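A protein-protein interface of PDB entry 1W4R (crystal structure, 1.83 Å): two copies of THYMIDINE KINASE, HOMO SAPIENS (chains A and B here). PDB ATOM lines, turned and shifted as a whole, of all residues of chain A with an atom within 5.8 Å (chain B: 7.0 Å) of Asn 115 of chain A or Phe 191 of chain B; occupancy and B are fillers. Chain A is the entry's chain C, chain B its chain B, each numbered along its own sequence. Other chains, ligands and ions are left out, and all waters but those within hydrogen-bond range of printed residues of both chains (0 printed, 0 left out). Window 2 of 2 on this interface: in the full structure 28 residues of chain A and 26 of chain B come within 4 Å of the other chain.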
ATOM      1  N   GLY A  20     -18.136   8.506 -10.335  1.00  0.00           N
ATOM      2  CA  GLY A  20     -17.164   7.581 -10.899  1.00  0.00           C
ATOM      3  C   GLY A  20     -17.093   6.274 -10.117  1.00  0.00           C
ATOM      4  O   GLY A  20     -17.373   6.242  -8.931  1.00  0.00           O
ATOM      5  N   CYS A 110      -7.266   2.996 -13.829  1.00  0.00           N
ATOM      6  CA  CYS A 110      -8.653   2.830 -13.396  1.00  0.00           C
ATOM      7  C   CYS A 110      -8.962   3.790 -12.270  1.00  0.00           C
ATOM      8  O   CYS A 110     -10.010   4.398 -12.255  1.00  0.00           O
ATOM      9  CB  CYS A 110      -8.885   1.386 -12.945  1.00  0.00           C
ATOM     10  SG  CYS A 110      -8.926   0.316 -14.379  1.00  0.00           S
ATOM     11  N   GLU A 111      -8.047   3.914 -11.327  1.00  0.00           N
ATOM     12  CA  GLU A 111      -8.241   4.807 -10.197  1.00  0.00           C
ATOM     13  C   GLU A 111      -8.342   6.265 -10.677  1.00  0.00           C
ATOM     14  O   GLU A 111      -9.240   6.978 -10.271  1.00  0.00           O
ATOM     15  CB  GLU A 111      -7.147   4.562  -9.151  1.00  0.00           C
ATOM     16  CG  GLU A 111      -7.165   5.414  -7.889  1.00  0.00           C
ATOM     17  CD  GLU A 111      -8.351   5.212  -6.960  1.00  0.00           C
ATOM     18  OE1 GLU A 111      -9.220   4.329  -7.179  1.00  0.00           O
ATOM     19  OE2 GLU A 111      -8.410   5.981  -5.974  1.00  0.00           O
ATOM     20  N   ALA A 112      -7.493   6.683 -11.618  1.00  0.00           N
ATOM     21  CA  ALA A 112      -7.537   8.068 -12.102  1.00  0.00           C
ATOM     22  C   ALA A 112      -8.818   8.381 -12.864  1.00  0.00           C
ATOM     23  O   ALA A 112      -9.439   9.425 -12.672  1.00  0.00           O
ATOM     24  CB  ALA A 112      -6.289   8.365 -12.988  1.00  0.00           C
ATOM     25  N   MET A 113      -9.249   7.460 -13.709  1.00  0.00           N
ATOM     26  CA  MET A 113     -10.485   7.649 -14.460  1.00  0.00           C
ATOM     27  C   MET A 113     -11.712   7.664 -13.563  1.00  0.00           C
ATOM     28  O   MET A 113     -12.596   8.486 -13.748  1.00  0.00           O
ATOM     29  CB  MET A 113     -10.617   6.592 -15.550  1.00  0.00           C
ATOM     30  CG  MET A 113      -9.513   6.686 -16.594  1.00  0.00           C
ATOM     31  SD  MET A 113      -9.675   8.281 -17.495  1.00  0.00           S
ATOM     32  CE  MET A 113      -8.037   8.416 -18.133  1.00  0.00           C
ATOM     33  N   ALA A 114     -11.767   6.766 -12.574  1.00  0.00           N
ATOM     34  CA  ALA A 114     -12.907   6.741 -11.674  1.00  0.00           C
ATOM     35  C   ALA A 114     -12.942   8.025 -10.837  1.00  0.00           C
ATOM     36  O   ALA A 114     -13.995   8.596 -10.614  1.00  0.00           O
ATOM     37  CB  ALA A 114     -12.851   5.485 -10.751  1.00  0.00           C
ATOM     38  N   ASN A 115     -11.779   8.457 -10.366  1.00  0.00           N
ATOM     39  CA  ASN A 115     -11.649   9.696  -9.599  1.00  0.00           C
ATOM     40  C   ASN A 115     -11.957  10.943 -10.450  1.00  0.00           C
ATOM     41  O   ASN A 115     -12.324  11.964  -9.904  1.00  0.00           O
ATOM     42  CB  ASN A 115     -10.260   9.770  -8.954  1.00  0.00           C
ATOM     43  CG  ASN A 115     -10.132   8.850  -7.751  1.00  0.00           C
ATOM     44  OD1 ASN A 115     -11.123   8.512  -7.116  1.00  0.00           O
ATOM     45  ND2 ASN A 115      -8.918   8.490  -7.409  1.00  0.00           N
ATOM     46  N   ALA A 116     -11.885  10.832 -11.778  1.00  0.00           N
ATOM     47  CA  ALA A 116     -12.341  11.882 -12.710  1.00  0.00           C
ATOM     48  C   ALA A 116     -13.801  11.726 -13.125  1.00  0.00           C
ATOM     49  O   ALA A 116     -14.264  12.428 -14.010  1.00  0.00           O
ATOM     50  CB  ALA A 116     -11.442  11.917 -13.950  1.00  0.00           C
ATOM     51  N   GLY A 117     -14.537  10.814 -12.478  1.00  0.00           N
ATOM     52  CA  GLY A 117     -15.964  10.668 -12.694  1.00  0.00           C
ATOM     53  C   GLY A 117     -16.428   9.600 -13.685  1.00  0.00           C
ATOM     54  O   GLY A 117     -17.610   9.506 -13.968  1.00  0.00           O
ATOM     55  N   LYS A 118     -15.517   8.791 -14.202  1.00  0.00           N
ATOM     56  CA  LYS A 118     -15.863   7.787 -15.202  1.00  0.00           C
ATOM     57  C   LYS A 118     -16.255   6.481 -14.509  1.00  0.00           C
ATOM     58  O   LYS A 118     -15.734   6.154 -13.466  1.00  0.00           O
ATOM     59  CB  LYS A 118     -14.675   7.514 -16.110  1.00  0.00           C
ATOM     60  CG  LYS A 118     -14.470   8.630 -17.182  1.00  0.00           C
ATOM     61  CD  LYS A 118     -13.397   9.585 -16.824  1.00  0.00           C
ATOM     62  CE  LYS A 118     -13.162  10.622 -17.969  1.00  0.00           C
ATOM     63  NZ  LYS A 118     -14.388  11.320 -18.502  1.00  0.00           N
ATOM     64  N   ARG B 131      -7.012   1.835   1.468  1.00  0.00           N
ATOM     65  CA  ARG B 131      -7.470   1.165   0.244  1.00  0.00           C
ATOM     66  C   ARG B 131      -6.346   0.417  -0.454  1.00  0.00           C
ATOM     67  O   ARG B 131      -6.275   0.389  -1.681  1.00  0.00           O
ATOM     68  CB  ARG B 131      -8.156   2.155  -0.716  1.00  0.00           C
ATOM     69  CG  ARG B 131      -9.480   2.657  -0.235  1.00  0.00           C
ATOM     70  CD  ARG B 131     -10.012   3.883  -0.931  1.00  0.00           C
ATOM     71  NE  ARG B 131     -10.535   3.590  -2.269  1.00  0.00           N
ATOM     72  CZ  ARG B 131     -10.024   4.037  -3.412  1.00  0.00           C
ATOM     73  NH1 ARG B 131     -10.613   3.702  -4.540  1.00  0.00           N
ATOM     74  NH2 ARG B 131      -8.952   4.821  -3.432  1.00  0.00           N
ATOM     75  N   TYR B 163     -15.583   1.201   0.835  1.00  0.00           N
ATOM     76  CA  TYR B 163     -14.325   1.442   1.518  1.00  0.00           C
ATOM     77  C   TYR B 163     -14.513   1.700   3.001  1.00  0.00           C
ATOM     78  O   TYR B 163     -15.609   1.969   3.456  1.00  0.00           O
ATOM     79  CB  TYR B 163     -13.570   2.634   0.868  1.00  0.00           C
ATOM     80  CG  TYR B 163     -13.650   2.588  -0.616  1.00  0.00           C
ATOM     81  CD1 TYR B 163     -13.058   1.553  -1.327  1.00  0.00           C
ATOM     82  CD2 TYR B 163     -14.408   3.513  -1.313  1.00  0.00           C
ATOM     83  CE1 TYR B 163     -13.215   1.458  -2.689  1.00  0.00           C
ATOM     84  CE2 TYR B 163     -14.574   3.428  -2.667  1.00  0.00           C
ATOM     85  CZ  TYR B 163     -13.961   2.407  -3.364  1.00  0.00           C
ATOM     86  OH  TYR B 163     -14.112   2.324  -4.735  1.00  0.00           O
ATOM     87  N   LYS B 165     -12.945   4.162   5.979  1.00  0.00           N
ATOM     88  CA  LYS B 165     -12.130   5.317   6.372  1.00  0.00           C
ATOM     89  C   LYS B 165     -11.853   5.230   7.866  1.00  0.00           C
ATOM     90  O   LYS B 165     -12.739   4.958   8.688  1.00  0.00           O
ATOM     91  CB  LYS B 165     -12.838   6.627   5.988  1.00  0.00           C
ATOM     92  CG  LYS B 165     -12.283   7.922   6.654  1.00  0.00           C
ATOM     93  CD  LYS B 165     -12.454   9.194   5.800  1.00  0.00           C
ATOM     94  CE  LYS B 165     -13.878   9.494   5.464  1.00  0.00           C
ATOM     95  NZ  LYS B 165     -14.146  10.972   5.256  1.00  0.00           N
ATOM     96  N   VAL B 185     -17.411   4.184   3.821  1.00  0.00           N
ATOM     97  CA  VAL B 185     -17.614   5.285   2.906  1.00  0.00           C
ATOM     98  C   VAL B 185     -17.566   4.896   1.452  1.00  0.00           C
ATOM     99  O   VAL B 185     -16.929   3.918   1.057  1.00  0.00           O
ATOM    100  CB  VAL B 185     -16.536   6.385   3.124  1.00  0.00           C
ATOM    101  CG1 VAL B 185     -16.742   7.047   4.460  1.00  0.00           C
ATOM    102  CG2 VAL B 185     -15.165   5.773   3.054  1.00  0.00           C
ATOM    103  N   CYS B 186     -18.203   5.734   0.660  1.00  0.00           N
ATOM    104  CA  CYS B 186     -18.113   5.724  -0.807  1.00  0.00           C
ATOM    105  C   CYS B 186     -16.822   6.421  -1.226  1.00  0.00           C
ATOM    106  O   CYS B 186     -16.080   6.942  -0.392  1.00  0.00           O
ATOM    107  CB  CYS B 186     -19.322   6.435  -1.409  1.00  0.00           C
ATOM    108  SG  CYS B 186     -19.366   8.236  -1.097  1.00  0.00           S
ATOM    109  N   ARG B 187     -16.566   6.444  -2.535  1.00  0.00           N
ATOM    110  CA  ARG B 187     -15.337   7.008  -3.078  1.00  0.00           C
ATOM    111  C   ARG B 187     -15.222   8.514  -2.779  1.00  0.00           C
ATOM    112  O   ARG B 187     -14.174   8.982  -2.341  1.00  0.00           O
ATOM    113  CB  ARG B 187     -15.311   6.760  -4.586  1.00  0.00           C
ATOM    114  CG  ARG B 187     -14.118   7.290  -5.361  1.00  0.00           C
ATOM    115  CD  ARG B 187     -14.323   7.027  -6.835  1.00  0.00           C
ATOM    116  NE  ARG B 187     -14.151   5.591  -7.064  1.00  0.00           N
ATOM    117  CZ  ARG B 187     -12.979   5.003  -7.182  1.00  0.00           C
ATOM    118  NH1 ARG B 187     -11.850   5.711  -7.174  1.00  0.00           N
ATOM    119  NH2 ARG B 187     -12.922   3.683  -7.340  1.00  0.00           N
ATOM    120  N   LEU B 188     -16.310   9.229  -2.987  1.00  0.00           N
ATOM    121  CA  LEU B 188     -16.290  10.686  -2.823  1.00  0.00           C
ATOM    122  C   LEU B 188     -16.068  11.021  -1.373  1.00  0.00           C
ATOM    123  O   LEU B 188     -15.211  11.850  -1.051  1.00  0.00           O
ATOM    124  CB  LEU B 188     -17.559  11.319  -3.368  1.00  0.00           C
ATOM    125  CG  LEU B 188     -17.748  11.228  -4.887  1.00  0.00           C
ATOM    126  CD1 LEU B 188     -19.047  11.912  -5.335  1.00  0.00           C
ATOM    127  CD2 LEU B 188     -16.546  11.836  -5.635  1.00  0.00           C
ATOM    128  N   CYS B 189     -16.789  10.360  -0.470  1.00  0.00           N
ATOM    129  CA  CYS B 189     -16.572  10.609   0.958  1.00  0.00           C
ATOM    130  C   CYS B 189     -15.212  10.179   1.458  1.00  0.00           C
ATOM    131  O   CYS B 189     -14.620  10.835   2.312  1.00  0.00           O
ATOM    132  CB  CYS B 189     -17.693  10.038   1.807  1.00  0.00           C
ATOM    133  SG  CYS B 189     -19.279  10.818   1.445  1.00  0.00           S
ATOM    134  N   TYR B 190     -14.669   9.110   0.892  1.00  0.00           N
ATOM    135  CA  TYR B 190     -13.344   8.671   1.275  1.00  0.00           C
ATOM    136  C   TYR B 190     -12.317   9.795   1.143  1.00  0.00           C
ATOM    137  O   TYR B 190     -11.462   9.926   1.998  1.00  0.00           O
ATOM    138  CB  TYR B 190     -12.872   7.459   0.435  1.00  0.00           C
ATOM    139  CG  TYR B 190     -11.540   6.934   0.871  1.00  0.00           C
ATOM    140  CD1 TYR B 190     -11.428   6.037   1.928  1.00  0.00           C
ATOM    141  CD2 TYR B 190     -10.374   7.311   0.225  1.00  0.00           C
ATOM    142  CE1 TYR B 190     -10.213   5.568   2.329  1.00  0.00           C
ATOM    143  CE2 TYR B 190      -9.148   6.844   0.631  1.00  0.00           C
ATOM    144  CZ  TYR B 190      -9.066   5.984   1.686  1.00  0.00           C
ATOM    145  OH  TYR B 190      -7.844   5.522   2.082  1.00  0.00           O
ATOM    146  N   PHE B 191     -12.430  10.582   0.079  1.00  0.00           N
ATOM    147  CA  PHE B 191     -11.417  11.567  -0.266  1.00  0.00           C
ATOM    148  C   PHE B 191     -11.637  13.060   0.123  1.00  0.00           C
ATOM    149  O   PHE B 191     -10.648  13.711   0.408  1.00  0.00           O
ATOM    150  CB  PHE B 191     -11.179  11.554  -1.829  1.00  0.00           C
ATOM    151  CG  PHE B 191     -10.379  10.370  -2.337  1.00  0.00           C
ATOM    152  CD1 PHE B 191     -10.933   9.474  -3.264  1.00  0.00           C
ATOM    153  CD2 PHE B 191      -9.084  10.142  -1.900  1.00  0.00           C
ATOM    154  CE1 PHE B 191     -10.215   8.389  -3.718  1.00  0.00           C
ATOM    155  CE2 PHE B 191      -8.360   9.052  -2.389  1.00  0.00           C
ATOM    156  CZ  PHE B 191      -8.950   8.173  -3.288  1.00  0.00           C
ATOM    157  N   LYS B 192     -12.834  13.609   0.333  1.00  0.00           N
ATOM    158  CA  LYS B 192     -13.363  14.034   1.651  1.00  0.00           C
ATOM    159  C   LYS B 192     -12.634  13.546   2.876  1.00  0.00           C
ATOM    160  O   LYS B 192     -12.055  14.369   3.558  1.00  0.00           O
ATOM    161  CB  LYS B 192     -14.883  13.880   1.782  1.00  0.00           C
ATOM    162  CG  LYS B 192     -15.671  15.073   1.270  1.00  0.00           C
ATOM    163  CD  LYS B 192     -17.156  15.021   1.685  1.00  0.00           C
ATOM    164  CE  LYS B 192     -17.353  15.144   3.220  1.00  0.00           C
ATOM    165  NZ  LYS B 192     -17.376  13.792   3.954  1.00  0.00           N
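Asn 115 of chain A touches two residues of chain B. Phe 191 of chain B touches just these residues of chain A: Glu 111 and Asn 115. Of the printed residues of chain B, Ala 114 of chain A touches Arg 187. Printed residues of chain A within 4 Å of Arg 187 of chain B: Gly 20 (3.8 Å), Glu 111 (3.0 Å), Ala 114 (3.6 Å) and Asn 115 (2.9 Å). Of the printed residues of chain B, Glu 111 of chain A touches Arg 131 (2.8 Å), Arg 187 (3.0 Å) and Phe 191 (3.5 Å). Leu 188 of chain B touches none of the printed residues of chain A. Lys 165 of chain B touches none of the printed residues of chain A. The nearest residue of chain B that does not touch Asn 115 of chain A is Arg 131 of chain B (5.4 Å). The nearest printed residue of chain A that does not touch Phe 191 of chain B is Ala 114 of chain A (7.6 Å).
No position is printed for both chains. Of the 7 pairs that touch across the chains among the printed residues, none has its exchanged pair printed and touching as well.
The guanidinium group of Arg 187 of chain B is in salt-bridge range of the side-chain carboxylate of Glu 111 of chain A (3.0 Å). NH1 of Arg 187 of chain B is in hydrogen-bond range of OD1 of Asn 115 of chain A. NH2 of Arg 131 of chain B is in salt-bridge range of OE2 of Glu 111 of chain A, at 2.8 Å.
Of the 10 printed residues of chain A, 4 touch a printed residue of chain B. Printed residues of chain A that touch a printed residue of chain B: Gly 20, Glu 111, Ala 114 and Asn 115. Along chain A the printed residues that touch a printed residue of chain B span positions 20 to 115. Of the 11 printed residues of chain B, 3 touch a printed residue of chain A. Among the printed residues, 7 pairs touch across the chains. Among the printed residues, Asp or Glu carboxylates within 4 Å of a Lys or Arg side-chain nitrogen of the other chain: Glu 111 of chain A with Arg 131 of chain B (2.8 Å) and Glu 111 of chain A with Arg 187 of chain B (3.0 Å).
Among the printed residues, pairs that only touch across the chains: Glu 111 of chain A with Phe 191 of chain B, Asn 115 of chain A with Phe 191 of chain B, Ala 114 of chain A with Arg 187 of chain B and Gly 20 of chain A with Arg 187 of chain B.
OE2 of Glu 111 of chain A sits at hydrogen-bond distance from ND2 of Asn 115 of chain A (2.9 Å). The side-chain hydroxyl (OH) of Tyr 163 of chain B lies within hydrogen-bond range of the guanidinium group (NH2) of Arg 187 of chain B, at 3.2 Å.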
